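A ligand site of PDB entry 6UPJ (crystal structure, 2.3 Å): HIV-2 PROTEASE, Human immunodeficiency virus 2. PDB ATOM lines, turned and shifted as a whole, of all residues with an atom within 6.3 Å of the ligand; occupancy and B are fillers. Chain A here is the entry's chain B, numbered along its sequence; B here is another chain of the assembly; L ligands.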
ATOM      1  N   LEU A  23     -30.229  -9.142 -16.059  1.00  0.00           N
ATOM      2  CA  LEU A  23     -29.744  -9.881 -17.236  1.00  0.00           C
ATOM      3  C   LEU A  23     -28.314 -10.330 -16.946  1.00  0.00           C
ATOM      4  O   LEU A  23     -27.515  -9.549 -16.437  1.00  0.00           O
ATOM      5  CB  LEU A  23     -29.735  -8.982 -18.475  1.00  0.00           C
ATOM      6  CG  LEU A  23     -29.431  -9.603 -19.847  1.00  0.00           C
ATOM      7  CD1 LEU A  23     -30.571 -10.519 -20.236  1.00  0.00           C
ATOM      8  CD2 LEU A  23     -29.219  -8.539 -20.923  1.00  0.00           C
ATOM      9  N   ASP A  25     -24.909 -10.896 -18.206  1.00  0.00           N
ATOM     10  CA  ASP A  25     -24.070 -10.413 -19.325  1.00  0.00           C
ATOM     11  C   ASP A  25     -22.588 -10.754 -19.210  1.00  0.00           C
ATOM     12  O   ASP A  25     -21.883 -10.116 -18.439  1.00  0.00           O
ATOM     13  CB  ASP A  25     -24.221  -8.890 -19.375  1.00  0.00           C
ATOM     14  CG  ASP A  25     -23.875  -8.310 -20.726  1.00  0.00           C
ATOM     15  OD1 ASP A  25     -23.048  -8.864 -21.490  1.00  0.00           O
ATOM     16  OD2 ASP A  25     -24.438  -7.241 -21.008  1.00  0.00           O
ATOM     17  N   GLY A  27     -20.356 -10.063 -21.398  1.00  0.00           N
ATOM     18  CA  GLY A  27     -19.551  -9.032 -22.014  1.00  0.00           C
ATOM     19  C   GLY A  27     -19.360  -7.844 -21.095  1.00  0.00           C
ATOM     20  O   GLY A  27     -18.687  -6.896 -21.439  1.00  0.00           O
ATOM     21  N   ALA A  28     -19.957  -7.877 -19.913  1.00  0.00           N
ATOM     22  CA  ALA A  28     -19.829  -6.756 -18.978  1.00  0.00           C
ATOM     23  C   ALA A  28     -18.841  -7.125 -17.907  1.00  0.00           C
ATOM     24  O   ALA A  28     -18.896  -8.235 -17.376  1.00  0.00           O
ATOM     25  CB  ALA A  28     -21.181  -6.409 -18.365  1.00  0.00           C
ATOM     26  N   ASP A  29     -17.932  -6.212 -17.600  1.00  0.00           N
ATOM     27  CA  ASP A  29     -16.917  -6.425 -16.574  1.00  0.00           C
ATOM     28  C   ASP A  29     -17.508  -6.238 -15.187  1.00  0.00           C
ATOM     29  O   ASP A  29     -17.126  -6.922 -14.233  1.00  0.00           O
ATOM     30  CB  ASP A  29     -15.752  -5.418 -16.723  1.00  0.00           C
ATOM     31  CG  ASP A  29     -14.874  -5.672 -17.958  1.00  0.00           C
ATOM     32  OD1 ASP A  29     -15.291  -6.368 -18.897  1.00  0.00           O
ATOM     33  OD2 ASP A  29     -13.748  -5.133 -18.000  1.00  0.00           O
ATOM     34  N   ASP A  30     -18.447  -5.302 -15.079  1.00  0.00           N
ATOM     35  CA  ASP A  30     -19.078  -4.953 -13.810  1.00  0.00           C
ATOM     36  C   ASP A  30     -20.597  -5.145 -13.789  1.00  0.00           C
ATOM     37  O   ASP A  30     -21.188  -5.543 -14.799  1.00  0.00           O
ATOM     38  CB  ASP A  30     -18.742  -3.491 -13.437  1.00  0.00           C
ATOM     39  CG  ASP A  30     -17.311  -3.091 -13.828  1.00  0.00           C
ATOM     40  OD1 ASP A  30     -16.365  -3.475 -13.111  1.00  0.00           O
ATOM     41  OD2 ASP A  30     -17.149  -2.400 -14.865  1.00  0.00           O
ATOM     42  N   ILE A  32     -24.308  -3.209 -12.831  1.00  0.00           N
ATOM     43  CA  ILE A  32     -24.998  -1.924 -12.644  1.00  0.00           C
ATOM     44  C   ILE A  32     -26.498  -2.218 -12.584  1.00  0.00           C
ATOM     45  O   ILE A  32     -26.986  -3.013 -13.368  1.00  0.00           O
ATOM     46  CB  ILE A  32     -24.778  -0.962 -13.891  1.00  0.00           C
ATOM     47  CG1 ILE A  32     -23.297  -0.782 -14.175  1.00  0.00           C
ATOM     48  CG2 ILE A  32     -25.400   0.422 -13.658  1.00  0.00           C
ATOM     49  CD1 ILE A  32     -23.022   0.084 -15.392  1.00  0.00           C
ATOM     50  N   VAL A  47     -18.643   4.791 -16.216  1.00  0.00           N
ATOM     51  CA  VAL A  47     -18.401   3.583 -17.004  1.00  0.00           C
ATOM     52  C   VAL A  47     -18.786   3.820 -18.429  1.00  0.00           C
ATOM     53  O   VAL A  47     -19.759   4.520 -18.700  1.00  0.00           O
ATOM     54  CB  VAL A  47     -19.168   2.346 -16.471  1.00  0.00           C
ATOM     55  CG1 VAL A  47     -20.670   2.468 -16.792  1.00  0.00           C
ATOM     56  CG2 VAL A  47     -18.607   1.047 -17.086  1.00  0.00           C
ATOM     57  N   GLY A  48     -18.040   3.219 -19.349  1.00  0.00           N
ATOM     58  CA  GLY A  48     -18.346   3.379 -20.752  1.00  0.00           C
ATOM     59  C   GLY A  48     -18.767   2.101 -21.435  1.00  0.00           C
ATOM     60  O   GLY A  48     -18.329   1.018 -21.079  1.00  0.00           O
ATOM     61  N   GLY A  49     -19.595   2.251 -22.453  1.00  0.00           N
ATOM     62  CA  GLY A  49     -20.059   1.121 -23.214  1.00  0.00           C
ATOM     63  C   GLY A  49     -20.469   1.641 -24.574  1.00  0.00           C
ATOM     64  O   GLY A  49     -20.032   2.714 -24.987  1.00  0.00           O
ATOM     65  N   ILE A  50     -21.319   0.905 -25.274  1.00  0.00           N
ATOM     66  CA  ILE A  50     -21.782   1.300 -26.589  1.00  0.00           C
ATOM     67  C   ILE A  50     -22.722   2.512 -26.495  1.00  0.00           C
ATOM     68  O   ILE A  50     -23.675   2.480 -25.732  1.00  0.00           O
ATOM     69  CB  ILE A  50     -22.488   0.120 -27.263  1.00  0.00           C
ATOM     70  CG1 ILE A  50     -21.480  -1.046 -27.382  1.00  0.00           C
ATOM     71  CG2 ILE A  50     -23.181   0.567 -28.578  1.00  0.00           C
ATOM     72  CD1 ILE A  50     -22.072  -2.337 -27.914  1.00  0.00           C
ATOM     73  N   GLY A  51     -22.405   3.568 -27.245  1.00  0.00           N
ATOM     74  CA  GLY A  51     -23.235   4.767 -27.237  1.00  0.00           C
ATOM     75  C   GLY A  51     -22.865   5.848 -26.221  1.00  0.00           C
ATOM     76  O   GLY A  51     -23.407   6.965 -26.280  1.00  0.00           O
ATOM     77  N   ILE A  54     -22.016   6.195 -18.409  1.00  0.00           N
ATOM     78  CA  ILE A  54     -23.041   6.252 -17.356  1.00  0.00           C
ATOM     79  C   ILE A  54     -22.271   6.559 -16.069  1.00  0.00           C
ATOM     80  O   ILE A  54     -21.186   5.995 -15.850  1.00  0.00           O
ATOM     81  CB  ILE A  54     -23.707   4.859 -17.082  1.00  0.00           C
ATOM     82  CG1 ILE A  54     -23.650   3.960 -18.303  1.00  0.00           C
ATOM     83  CG2 ILE A  54     -25.171   5.028 -16.649  1.00  0.00           C
ATOM     84  CD1 ILE A  54     -24.221   2.623 -18.003  1.00  0.00           C
ATOM     85  N   PRO A  81     -30.456   1.439 -18.818  1.00  0.00           N
ATOM     86  CA  PRO A  81     -31.775   1.093 -19.371  1.00  0.00           C
ATOM     87  C   PRO A  81     -32.211  -0.352 -19.097  1.00  0.00           C
ATOM     88  O   PRO A  81     -33.361  -0.732 -19.353  1.00  0.00           O
ATOM     89  CB  PRO A  81     -31.601   1.349 -20.859  1.00  0.00           C
ATOM     90  CG  PRO A  81     -30.163   0.963 -21.088  1.00  0.00           C
ATOM     91  CD  PRO A  81     -29.445   1.582 -19.886  1.00  0.00           C
ATOM     92  N   ILE A  82     -31.278  -1.149 -18.560  1.00  0.00           N
ATOM     93  CA  ILE A  82     -31.526  -2.550 -18.286  1.00  0.00           C
ATOM     94  C   ILE A  82     -30.541  -2.934 -17.186  1.00  0.00           C
ATOM     95  O   ILE A  82     -29.382  -2.539 -17.229  1.00  0.00           O
ATOM     96  CB  ILE A  82     -31.303  -3.373 -19.597  1.00  0.00           C
ATOM     97  CG1 ILE A  82     -31.275  -4.893 -19.342  1.00  0.00           C
ATOM     98  CG2 ILE A  82     -30.040  -2.874 -20.334  1.00  0.00           C
ATOM     99  CD1 ILE A  82     -32.601  -5.506 -18.941  1.00  0.00           C
ATOM    100  N   ILE A  84     -27.943  -5.065 -15.167  1.00  0.00           N
ATOM    101  CA  ILE A  84     -26.930  -6.048 -15.553  1.00  0.00           C
ATOM    102  C   ILE A  84     -26.115  -6.710 -14.437  1.00  0.00           C
ATOM    103  O   ILE A  84     -25.746  -6.069 -13.452  1.00  0.00           O
ATOM    104  CB  ILE A  84     -25.881  -5.393 -16.497  1.00  0.00           C
ATOM    105  CG1 ILE A  84     -26.586  -4.528 -17.542  1.00  0.00           C
ATOM    106  CG2 ILE A  84     -25.024  -6.449 -17.162  1.00  0.00           C
ATOM    107  CD1 ILE A  84     -25.788  -4.322 -18.800  1.00  0.00           C
ATOM    108  N   ARG B   8     -12.104 -11.624 -20.271  1.00  0.00           N
ATOM    109  CA  ARG B   8     -13.040 -11.450 -21.384  1.00  0.00           C
ATOM    110  C   ARG B   8     -12.986 -12.560 -22.400  1.00  0.00           C
ATOM    111  O   ARG B   8     -11.926 -12.882 -22.937  1.00  0.00           O
ATOM    112  CB  ARG B   8     -12.819 -10.092 -22.051  1.00  0.00           C
ATOM    113  CG  ARG B   8     -13.145  -8.954 -21.088  1.00  0.00           C
ATOM    114  CD  ARG B   8     -12.345  -7.684 -21.359  1.00  0.00           C
ATOM    115  NE  ARG B   8     -12.992  -6.887 -22.383  1.00  0.00           N
ATOM    116  CZ  ARG B   8     -13.335  -5.619 -22.228  1.00  0.00           C
ATOM    117  NH1 ARG B   8     -13.103  -5.001 -21.080  1.00  0.00           N
ATOM    118  NH2 ARG B   8     -13.967  -4.994 -23.215  1.00  0.00           N
ATOM    119  N   LEU B  23     -15.893 -10.244 -28.725  1.00  0.00           N
ATOM    120  CA  LEU B  23     -16.214 -10.656 -27.369  1.00  0.00           C
ATOM    121  C   LEU B  23     -17.631 -11.237 -27.392  1.00  0.00           C
ATOM    122  O   LEU B  23     -18.578 -10.570 -27.813  1.00  0.00           O
ATOM    123  CB  LEU B  23     -16.159  -9.415 -26.485  1.00  0.00           C
ATOM    124  CG  LEU B  23     -16.667  -9.221 -25.063  1.00  0.00           C
ATOM    125  CD1 LEU B  23     -15.656  -9.703 -24.043  1.00  0.00           C
ATOM    126  CD2 LEU B  23     -16.894  -7.720 -24.897  1.00  0.00           C
ATOM    127  N   ASP B  25     -21.021 -11.918 -26.212  1.00  0.00           N
ATOM    128  CA  ASP B  25     -21.929 -11.206 -25.298  1.00  0.00           C
ATOM    129  C   ASP B  25     -23.300 -11.902 -25.122  1.00  0.00           C
ATOM    130  O   ASP B  25     -24.129 -11.882 -26.023  1.00  0.00           O
ATOM    131  CB  ASP B  25     -22.127  -9.800 -25.875  1.00  0.00           C
ATOM    132  CG  ASP B  25     -22.699  -8.809 -24.887  1.00  0.00           C
ATOM    133  OD1 ASP B  25     -23.669  -9.108 -24.180  1.00  0.00           O
ATOM    134  OD2 ASP B  25     -22.186  -7.675 -24.864  1.00  0.00           O
ATOM    135  N   GLY B  27     -25.753 -10.924 -23.235  1.00  0.00           N
ATOM    136  CA  GLY B  27     -26.840 -10.020 -22.896  1.00  0.00           C
ATOM    137  C   GLY B  27     -27.419  -9.273 -24.077  1.00  0.00           C
ATOM    138  O   GLY B  27     -28.480  -8.669 -23.984  1.00  0.00           O
ATOM    139  N   ALA B  28     -26.709  -9.313 -25.195  1.00  0.00           N
ATOM    140  CA  ALA B  28     -27.107  -8.634 -26.420  1.00  0.00           C
ATOM    141  C   ALA B  28     -27.940  -9.558 -27.305  1.00  0.00           C
ATOM    142  O   ALA B  28     -27.683 -10.765 -27.371  1.00  0.00           O
ATOM    143  CB  ALA B  28     -25.867  -8.168 -27.179  1.00  0.00           C
ATOM    144  N   ASP B  29     -28.879  -8.982 -28.038  1.00  0.00           N
ATOM    145  CA  ASP B  29     -29.746  -9.762 -28.910  1.00  0.00           C
ATOM    146  C   ASP B  29     -29.200  -9.896 -30.309  1.00  0.00           C
ATOM    147  O   ASP B  29     -29.507 -10.877 -30.989  1.00  0.00           O
ATOM    148  CB  ASP B  29     -31.131  -9.152 -29.003  1.00  0.00           C
ATOM    149  CG  ASP B  29     -31.886  -9.213 -27.689  1.00  0.00           C
ATOM    150  OD1 ASP B  29     -31.533 -10.042 -26.811  1.00  0.00           O
ATOM    151  OD2 ASP B  29     -32.830  -8.427 -27.556  1.00  0.00           O
ATOM    152  N   GLY B  48     -29.574   0.720 -29.898  1.00  0.00           N
ATOM    153  CA  GLY B  48     -29.475   1.358 -28.606  1.00  0.00           C
ATOM    154  C   GLY B  48     -28.475   0.639 -27.734  1.00  0.00           C
ATOM    155  O   GLY B  48     -28.600  -0.564 -27.499  1.00  0.00           O
ATOM    156  N   GLY B  49     -27.451   1.363 -27.275  1.00  0.00           N
ATOM    157  CA  GLY B  49     -26.471   0.746 -26.421  1.00  0.00           C
ATOM    158  C   GLY B  49     -26.803   1.105 -24.997  1.00  0.00           C
ATOM    159  O   GLY B  49     -27.853   1.696 -24.723  1.00  0.00           O
ATOM    160  N   ILE B  50     -25.884   0.767 -24.089  1.00  0.00           N
ATOM    161  CA  ILE B  50     -26.036   1.058 -22.687  1.00  0.00           C
ATOM    162  C   ILE B  50     -25.813   2.539 -22.450  1.00  0.00           C
ATOM    163  O   ILE B  50     -26.363   3.112 -21.511  1.00  0.00           O
ATOM    164  CB  ILE B  50     -25.032   0.249 -21.866  1.00  0.00           C
ATOM    165  CG1 ILE B  50     -25.601  -0.034 -20.479  1.00  0.00           C
ATOM    166  CG2 ILE B  50     -23.700   0.982 -21.763  1.00  0.00           C
ATOM    167  CD1 ILE B  50     -26.769  -0.994 -20.479  1.00  0.00           C
ATOM    168  N   GLY B  51     -24.992   3.157 -23.276  1.00  0.00           N
ATOM    169  CA  GLY B  51     -24.707   4.572 -23.117  1.00  0.00           C
ATOM    170  C   GLY B  51     -25.596   5.494 -23.929  1.00  0.00           C
ATOM    171  O   GLY B  51     -25.874   6.637 -23.525  1.00  0.00           O
ATOM    172  N   ILE B  82     -16.483  -1.538 -29.193  1.00  0.00           N
ATOM    173  CA  ILE B  82     -16.187  -2.930 -28.852  1.00  0.00           C
ATOM    174  C   ILE B  82     -16.984  -3.811 -29.844  1.00  0.00           C
ATOM    175  O   ILE B  82     -18.113  -3.473 -30.211  1.00  0.00           O
ATOM    176  CB  ILE B  82     -16.494  -3.235 -27.322  1.00  0.00           C
ATOM    177  CG1 ILE B  82     -15.403  -4.158 -26.720  1.00  0.00           C
ATOM    178  CG2 ILE B  82     -17.885  -3.802 -27.114  1.00  0.00           C
ATOM    179  CD1 ILE B  82     -15.289  -5.553 -27.340  1.00  0.00           C
ATOM    180  N   ILE B  84     -18.928  -7.129 -30.831  1.00  0.00           N
ATOM    181  CA  ILE B  84     -19.647  -8.176 -30.110  1.00  0.00           C
ATOM    182  C   ILE B  84     -20.439  -9.131 -31.013  1.00  0.00           C
ATOM    183  O   ILE B  84     -20.865  -8.779 -32.127  1.00  0.00           O
ATOM    184  CB  ILE B  84     -20.638  -7.626 -29.024  1.00  0.00           C
ATOM    185  CG1 ILE B  84     -21.671  -6.706 -29.663  1.00  0.00           C
ATOM    186  CG2 ILE B  84     -19.878  -6.960 -27.879  1.00  0.00           C
ATOM    187  CD1 ILE B  84     -22.993  -6.621 -28.884  1.00  0.00           C
HETATM  188  C1  LIG L   1     -22.930  -3.807 -23.384  1.00  0.00           C
HETATM  189  C2  LIG L   1     -23.230  -2.529 -23.959  1.00  0.00           C
HETATM  190  O1  LIG L   1     -22.498  -1.613 -23.801  1.00  0.00           O
HETATM  191  O2  LIG L   1     -24.365  -2.281 -24.649  1.00  0.00           O
HETATM  192  C3  LIG L   1     -25.245  -3.364 -24.789  1.00  0.00           C
HETATM  193  C4  LIG L   1     -25.022  -4.656 -24.268  1.00  0.00           C
HETATM  194  C5  LIG L   1     -23.820  -4.846 -23.553  1.00  0.00           C
HETATM  195  O3  LIG L   1     -23.472  -6.070 -23.005  1.00  0.00           O
HETATM  196  C6  LIG L   1     -21.553  -3.118 -21.287  1.00  0.00           C
HETATM  197  C7  LIG L   1     -22.376  -3.361 -20.162  1.00  0.00           C
HETATM  198  C8  LIG L   1     -22.257  -2.535 -19.024  1.00  0.00           C
HETATM  199  C9  LIG L   1     -21.330  -1.467 -19.003  1.00  0.00           C
HETATM  200  C10 LIG L   1     -20.523  -1.237 -20.120  1.00  0.00           C
HETATM  201  C11 LIG L   1     -20.625  -2.035 -21.266  1.00  0.00           C
HETATM  202  C12 LIG L   1     -21.667  -4.033 -22.517  1.00  0.00           C
HETATM  203  C13 LIG L   1     -20.363  -4.280 -23.300  1.00  0.00           C
HETATM  204  C14 LIG L   1     -19.794  -3.086 -24.075  1.00  0.00           C
HETATM  205  C15 LIG L   1     -26.518  -3.026 -25.584  1.00  0.00           C
HETATM  206  C16 LIG L   1     -27.875  -3.344 -24.977  1.00  0.00           C
HETATM  207  C17 LIG L   1     -27.850  -4.079 -23.622  1.00  0.00           C
HETATM  208  C18 LIG L   1     -27.342  -5.532 -23.652  1.00  0.00           C
HETATM  209  C19 LIG L   1     -26.036  -5.764 -24.445  1.00  0.00           C
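The side-chain carboxylate (OD1) of Asp 25 of chain A lies within hydrogen-bond range of the backbone NH (N) of Gly 27 of chain A (2.9 Å).
The side-chain carboxylate (OD1) of Asp 25 of chain B sits at hydrogen-bond distance from the backbone NH (N) of Gly 27 of chain B, 2.9 Å away.
The side-chain carboxylate (OD1) of Asp 25 of chain B sits at hydrogen-bond distance from the backbone NH (N) of Ala 28 of chain B (3.2 Å).
N of Ile 50 of chain B sits at hydrogen-bond distance from O of Ile 50 of chain A.
The backbone NH of Gly 51 of chain B lies within hydrogen-bond range of the backbone carbonyl oxygen of Ile 50 of chain A, 2.9 Å away.
The backbone NH of Ile 84 of chain A sits at hydrogen-bond distance from the backbone carbonyl oxygen of Ile 32 (2.9 Å).
OD2 of Asp 25 of chain A is in hydrogen-bond range of O3 of the ligand (2.5 Å).
OD2 of Asp 25 of chain B lies within hydrogen-bond range of O3 of the ligand (2.8 Å).
The backbone NH (N) of Ile 50 of chain A is in hydrogen-bond range of an oxygen (O1) of the ligand (3.1 Å).
The backbone NH (N) of Ile 50 of chain B lies within hydrogen-bond range of an oxygen (O2) of the ligand (3.5 Å).
Residues that only touch the ligand: Gly 48 of chain A, Gly 27 of chain B, Gly 27 of chain A, Ala 28 of chain B, Ile 82 of chain B, Gly 49 of chain A, Ala 28 of chain A, Gly 48 of chain B, Ile 84 of chain A and Gly 49 of chain B.
Hydrophobic or aromatic side chains that line the ligand: Ala 28 of chain A, Ile 50 of chain A, Ile 84 of chain A, Ala 28 of chain B, Ile 50 of chain B and Ile 82 of chain B.
Of the 28 residues printed, 14 come within 4 Å of the ligand.
The nearest printed residue that does not touch the ligand is Ile 82 of chain A (4.1 Å).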
